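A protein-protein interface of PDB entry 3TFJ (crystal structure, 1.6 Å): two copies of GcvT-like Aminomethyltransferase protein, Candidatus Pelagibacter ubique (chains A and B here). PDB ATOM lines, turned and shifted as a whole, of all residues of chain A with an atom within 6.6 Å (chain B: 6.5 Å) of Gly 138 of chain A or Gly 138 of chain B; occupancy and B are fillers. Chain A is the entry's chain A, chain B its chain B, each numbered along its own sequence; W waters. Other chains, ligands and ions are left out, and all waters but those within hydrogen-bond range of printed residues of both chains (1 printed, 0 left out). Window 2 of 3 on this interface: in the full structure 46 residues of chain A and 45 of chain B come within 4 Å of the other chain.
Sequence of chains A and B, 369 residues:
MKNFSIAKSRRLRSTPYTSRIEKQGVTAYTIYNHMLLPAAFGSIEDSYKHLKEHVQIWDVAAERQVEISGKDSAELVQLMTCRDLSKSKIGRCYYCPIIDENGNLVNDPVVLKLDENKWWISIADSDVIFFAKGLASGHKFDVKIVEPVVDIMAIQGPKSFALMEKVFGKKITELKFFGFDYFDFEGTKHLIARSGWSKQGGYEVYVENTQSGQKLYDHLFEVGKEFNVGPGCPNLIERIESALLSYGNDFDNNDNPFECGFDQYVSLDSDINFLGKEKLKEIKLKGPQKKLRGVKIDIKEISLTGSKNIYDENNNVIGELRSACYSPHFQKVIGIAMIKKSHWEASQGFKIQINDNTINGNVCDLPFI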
ATOM      1  N   LYS A 133       9.004  27.828 -20.895  1.00  0.00           N
ATOM      2  CA  LYS A 133       7.858  26.911 -21.132  1.00  0.00           C
ATOM      3  C   LYS A 133       7.308  27.081 -22.559  1.00  0.00           C
ATOM      4  O   LYS A 133       6.935  26.111 -23.241  1.00  0.00           O
ATOM      5  CB  LYS A 133       6.711  27.057 -20.127  1.00  0.00           C
ATOM      6  CG  LYS A 133       7.050  26.491 -18.741  1.00  0.00           C
ATOM      7  CD  LYS A 133       6.128  27.023 -17.681  1.00  0.00           C
ATOM      8  CE  LYS A 133       6.294  26.346 -16.341  1.00  0.00           C
ATOM      9  NZ  LYS A 133       5.513  25.091 -16.196  1.00  0.00           N
ATOM     10  N   GLY A 134       7.117  28.317 -22.969  1.00  0.00           N
ATOM     11  CA  GLY A 134       6.670  28.585 -24.361  1.00  0.00           C
ATOM     12  C   GLY A 134       7.599  28.025 -25.408  1.00  0.00           C
ATOM     13  O   GLY A 134       7.129  27.342 -26.359  1.00  0.00           O
ATOM     14  N   LEU A 135       8.908  28.281 -25.236  1.00  0.00           N
ATOM     15  CA  LEU A 135       9.981  27.769 -26.137  1.00  0.00           C
ATOM     16  C   LEU A 135       9.994  26.254 -26.174  1.00  0.00           C
ATOM     17  O   LEU A 135      10.018  25.639 -27.262  1.00  0.00           O
ATOM     18  CB  LEU A 135      11.367  28.323 -25.808  1.00  0.00           C
ATOM     19  CG  LEU A 135      11.625  29.801 -26.130  1.00  0.00           C
ATOM     20  CD1 LEU A 135      12.891  30.245 -25.405  1.00  0.00           C
ATOM     21  CD2 LEU A 135      11.728  30.091 -27.618  1.00  0.00           C
ATOM     22  N   ALA A 136       9.934  25.630 -24.999  1.00  0.00           N
ATOM     23  CA  ALA A 136       9.963  24.198 -24.939  1.00  0.00           C
ATOM     24  C   ALA A 136       8.740  23.562 -25.651  1.00  0.00           C
ATOM     25  O   ALA A 136       8.886  22.535 -26.374  1.00  0.00           O
ATOM     26  CB  ALA A 136      10.041  23.742 -23.443  1.00  0.00           C
ATOM     27  N   SER A 137       7.535  24.096 -25.427  1.00  0.00           N
ATOM     28  CA  SER A 137       6.339  23.597 -26.076  1.00  0.00           C
ATOM     29  C   SER A 137       6.441  23.754 -27.602  1.00  0.00           C
ATOM     30  O   SER A 137       6.161  22.806 -28.386  1.00  0.00           O
ATOM     31  CB  SER A 137       5.112  24.320 -25.569  1.00  0.00           C
ATOM     32  OG  SER A 137       3.913  23.865 -26.199  1.00  0.00           O
ATOM     33  N   GLY A 138       6.830  24.931 -28.066  1.00  0.00           N
ATOM     34  CA  GLY A 138       6.911  25.149 -29.495  1.00  0.00           C
ATOM     35  C   GLY A 138       7.981  24.372 -30.242  1.00  0.00           C
ATOM     36  O   GLY A 138       7.795  24.031 -31.408  1.00  0.00           O
ATOM     37  N   HIS A 139       9.120  24.174 -29.589  1.00  0.00           N
ATOM     38  CA  HIS A 139      10.260  23.397 -30.079  1.00  0.00           C
ATOM     39  C   HIS A 139      10.119  21.889 -29.768  1.00  0.00           C
ATOM     40  O   HIS A 139      10.945  21.070 -30.216  1.00  0.00           O
ATOM     41  CB  HIS A 139      11.580  23.992 -29.564  1.00  0.00           C
ATOM     42  CG  HIS A 139      11.958  25.334 -30.170  1.00  0.00           C
ATOM     43  ND1 HIS A 139      12.833  25.426 -31.234  1.00  0.00           N
ATOM     44  CD2 HIS A 139      11.598  26.610 -29.881  1.00  0.00           C
ATOM     45  CE1 HIS A 139      12.998  26.693 -31.571  1.00  0.00           C
ATOM     46  NE2 HIS A 139      12.252  27.439 -30.775  1.00  0.00           N
ATOM     47  N   LYS A 140       9.050  21.498 -29.088  1.00  0.00           N
ATOM     48  CA  LYS A 140       8.842  20.121 -28.625  1.00  0.00           C
ATOM     49  C   LYS A 140      10.095  19.520 -27.939  1.00  0.00           C
ATOM     50  O   LYS A 140      10.472  18.359 -28.160  1.00  0.00           O
ATOM     51  CB  LYS A 140       8.280  19.247 -29.764  1.00  0.00           C
ATOM     52  CG  LYS A 140       6.764  19.552 -30.091  1.00  0.00           C
ATOM     53  CD  LYS A 140       6.199  18.840 -31.362  1.00  0.00           C
ATOM     54  CE  LYS A 140       5.024  19.609 -32.036  1.00  0.00           C
ATOM     55  NZ  LYS A 140       5.430  20.199 -33.374  1.00  0.00           N
ATOM     56  N   PHE A 141      10.745  20.321 -27.062  1.00  0.00           N
ATOM     57  CA  PHE A 141      11.905  19.900 -26.307  1.00  0.00           C
ATOM     58  C   PHE A 141      11.463  18.936 -25.181  1.00  0.00           C
ATOM     59  O   PHE A 141      10.397  19.038 -24.629  1.00  0.00           O
ATOM     60  CB  PHE A 141      12.691  21.069 -25.697  1.00  0.00           C
ATOM     61  CG  PHE A 141      13.493  21.864 -26.663  1.00  0.00           C
ATOM     62  CD1 PHE A 141      14.166  21.299 -27.717  1.00  0.00           C
ATOM     63  CD2 PHE A 141      13.547  23.228 -26.535  1.00  0.00           C
ATOM     64  CE1 PHE A 141      14.949  22.088 -28.561  1.00  0.00           C
ATOM     65  CE2 PHE A 141      14.363  24.001 -27.341  1.00  0.00           C
ATOM     66  CZ  PHE A 141      15.011  23.442 -28.396  1.00  0.00           C
ATOM     67  N   LYS B 133       5.730  34.849 -26.927  1.00  0.00           N
ATOM     68  CA  LYS B 133       6.930  34.941 -27.738  1.00  0.00           C
ATOM     69  C   LYS B 133       7.624  33.580 -27.844  1.00  0.00           C
ATOM     70  O   LYS B 133       8.102  33.204 -28.891  1.00  0.00           O
ATOM     71  CB  LYS B 133       7.888  36.010 -27.161  1.00  0.00           C
ATOM     72  CG  LYS B 133       7.446  37.463 -27.419  1.00  0.00           C
ATOM     73  CD  LYS B 133       8.338  38.428 -26.608  1.00  0.00           C
ATOM     74  CE  LYS B 133       8.071  39.841 -26.984  1.00  0.00           C
ATOM     75  NZ  LYS B 133       8.987  40.287 -28.051  1.00  0.00           N
ATOM     76  N   GLY B 134       7.673  32.868 -26.732  1.00  0.00           N
ATOM     77  CA  GLY B 134       8.283  31.529 -26.726  1.00  0.00           C
ATOM     78  C   GLY B 134       7.582  30.603 -27.665  1.00  0.00           C
ATOM     79  O   GLY B 134       8.243  29.938 -28.502  1.00  0.00           O
ATOM     80  N   LEU B 135       6.261  30.535 -27.505  1.00  0.00           N
ATOM     81  CA  LEU B 135       5.433  29.662 -28.388  1.00  0.00           C
ATOM     82  C   LEU B 135       5.604  30.064 -29.841  1.00  0.00           C
ATOM     83  O   LEU B 135       5.730  29.196 -30.716  1.00  0.00           O
ATOM     84  CB  LEU B 135       3.957  29.693 -27.966  1.00  0.00           C
ATOM     85  CG  LEU B 135       3.548  29.039 -26.647  1.00  0.00           C
ATOM     86  CD1 LEU B 135       2.148  29.469 -26.103  1.00  0.00           C
ATOM     87  CD2 LEU B 135       3.649  27.459 -26.731  1.00  0.00           C
ATOM     88  N   ALA B 136       5.574  31.363 -30.132  1.00  0.00           N
ATOM     89  CA  ALA B 136       5.630  31.855 -31.507  1.00  0.00           C
ATOM     90  C   ALA B 136       6.948  31.506 -32.184  1.00  0.00           C
ATOM     91  O   ALA B 136       6.977  31.149 -33.360  1.00  0.00           O
ATOM     92  CB  ALA B 136       5.378  33.382 -31.515  1.00  0.00           C
ATOM     93  N   SER B 137       8.044  31.534 -31.414  1.00  0.00           N
ATOM     94  CA  SER B 137       9.361  31.178 -31.909  1.00  0.00           C
ATOM     95  C   SER B 137       9.442  29.711 -32.275  1.00  0.00           C
ATOM     96  O   SER B 137       9.946  29.371 -33.350  1.00  0.00           O
ATOM     97  CB  SER B 137      10.423  31.539 -30.844  1.00  0.00           C
ATOM     98  OG  SER B 137      11.696  31.034 -31.179  1.00  0.00           O
ATOM     99  N   GLY B 138       8.881  28.859 -31.427  1.00  0.00           N
ATOM    100  CA  GLY B 138       8.921  27.406 -31.657  1.00  0.00           C
ATOM    101  C   GLY B 138       8.069  26.962 -32.839  1.00  0.00           C
ATOM    102  O   GLY B 138       8.478  26.106 -33.658  1.00  0.00           O
ATOM    103  N   HIS B 139       6.918  27.618 -33.000  1.00  0.00           N
ATOM    104  CA  HIS B 139       5.974  27.301 -34.092  1.00  0.00           C
ATOM    105  C   HIS B 139       6.308  28.066 -35.351  1.00  0.00           C
ATOM    106  O   HIS B 139       5.717  27.757 -36.395  1.00  0.00           O
ATOM    107  CB  HIS B 139       4.537  27.587 -33.649  1.00  0.00           C
ATOM    108  CG  HIS B 139       3.980  26.546 -32.724  1.00  0.00           C
ATOM    109  ND1 HIS B 139       3.549  25.331 -33.188  1.00  0.00           N
ATOM    110  CD2 HIS B 139       3.821  26.511 -31.372  1.00  0.00           C
ATOM    111  CE1 HIS B 139       3.135  24.591 -32.176  1.00  0.00           C
ATOM    112  NE2 HIS B 139       3.291  25.275 -31.063  1.00  0.00           N
ATOM    113  N   LYS B 140       7.259  29.017 -35.299  1.00  0.00           N
ATOM    114  CA  LYS B 140       7.546  29.895 -36.446  1.00  0.00           C
ATOM    115  C   LYS B 140       6.257  30.572 -36.910  1.00  0.00           C
ATOM    116  O   LYS B 140       6.009  30.717 -38.133  1.00  0.00           O
ATOM    117  CB  LYS B 140       8.226  29.123 -37.571  1.00  0.00           C
ATOM    118  CG  LYS B 140       9.417  28.312 -37.070  1.00  0.00           C
ATOM    119  CD  LYS B 140      10.169  27.585 -38.192  1.00  0.00           C
ATOM    120  CE  LYS B 140      11.559  27.192 -37.699  1.00  0.00           C
ATOM    121  NZ  LYS B 140      12.441  26.692 -38.771  1.00  0.00           N
ATOM    122  N   PHE B 141       5.425  30.995 -35.955  1.00  0.00           N
ATOM    123  CA  PHE B 141       4.174  31.661 -36.317  1.00  0.00           C
ATOM    124  C   PHE B 141       4.442  33.012 -36.924  1.00  0.00           C
ATOM    125  O   PHE B 141       5.389  33.733 -36.548  1.00  0.00           O
ATOM    126  CB  PHE B 141       3.287  31.876 -35.092  1.00  0.00           C
ATOM    127  CG  PHE B 141       2.537  30.671 -34.633  1.00  0.00           C
ATOM    128  CD1 PHE B 141       2.046  29.731 -35.535  1.00  0.00           C
ATOM    129  CD2 PHE B 141       2.265  30.495 -33.281  1.00  0.00           C
ATOM    130  CE1 PHE B 141       1.283  28.664 -35.088  1.00  0.00           C
ATOM    131  CE2 PHE B 141       1.545  29.376 -32.812  1.00  0.00           C
ATOM    132  CZ  PHE B 141       1.059  28.443 -33.747  1.00  0.00           C
HETATM  133  O   HOH W   1       2.783  24.181 -28.652  1.00  0.00           O
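Of the printed residues of chain B, Leu 135 of chain A touches Gly 134 (3.6 Å) and Ser 137 (3.7 Å). Phe 141 of chain A touches none of the printed residues of chain B. Lys 133 of chain B touches none of the printed residues of chain A. Of the printed residues of chain A, His 139 of chain B touches Gly 138. The nearest printed residue of chain B that does not touch Ser 137 of chain A is His 139 of chain B (4.6 Å).
Along chain A the printed residues that touch a printed residue of chain B span positions 134 to 139. Printed residues of chain B that touch a printed residue of chain A: Gly 134, Leu 135, Ser 137, Gly 138 and His 139. Hydrophobic or aromatic side chains of chain B within 4 Å of the printed part of chain A: Leu 135 and His 139. Among the printed residues, 9 pairs touch across the chains.
The backbone carbonyl oxygen (O) of Gly 138 of chain A sits close to the backbone carbonyl oxygen (O) of Gly 138 of chain B, at 3.1 Å.
Water W1 bridges NE2 of His 139 of chain B (2.7 Å) and OG of Ser 137 of chain A (2.7 Å).
Gly 134 of chain A touches its own counterpart, Gly 134 of chain B. Gly 134 of chain A touches Leu 135 of chain B, and with the chains exchanged Leu 135 of chain A touches Gly 134 of chain B. Leu 135 of chain A touches Ser 137 of chain B, and with the chains exchanged Ser 137 of chain A touches Leu 135 of chain B. Gly 138 of chain A touches His 139 of chain B, and with the chains exchanged His 139 of chain A touches Gly 138 of chain B. Positions printed for both chains: 133, 134, 135, 136, 137, 138, 139, 140 and 141.
Among the printed residues, merely in contact across the chains: Gly 134 of chain A with Gly 134 of chain B (3.4 Å), Gly 134 of chain A with Leu 135 of chain B (3.5 Å), Leu 135 of chain A with Gly 134 of chain B (3.6 Å), Leu 135 of chain A with Ser 137 of chain B (3.7 Å), Ser 137 of chain A with Leu 135 of chain B (3.6 Å), Gly 138 of chain A with His 139 of chain B (3.9 Å), His 139 of chain A with Ser 137 of chain B (3.7 Å) and His 139 of chain A with Gly 138 of chain B (3.3 Å).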
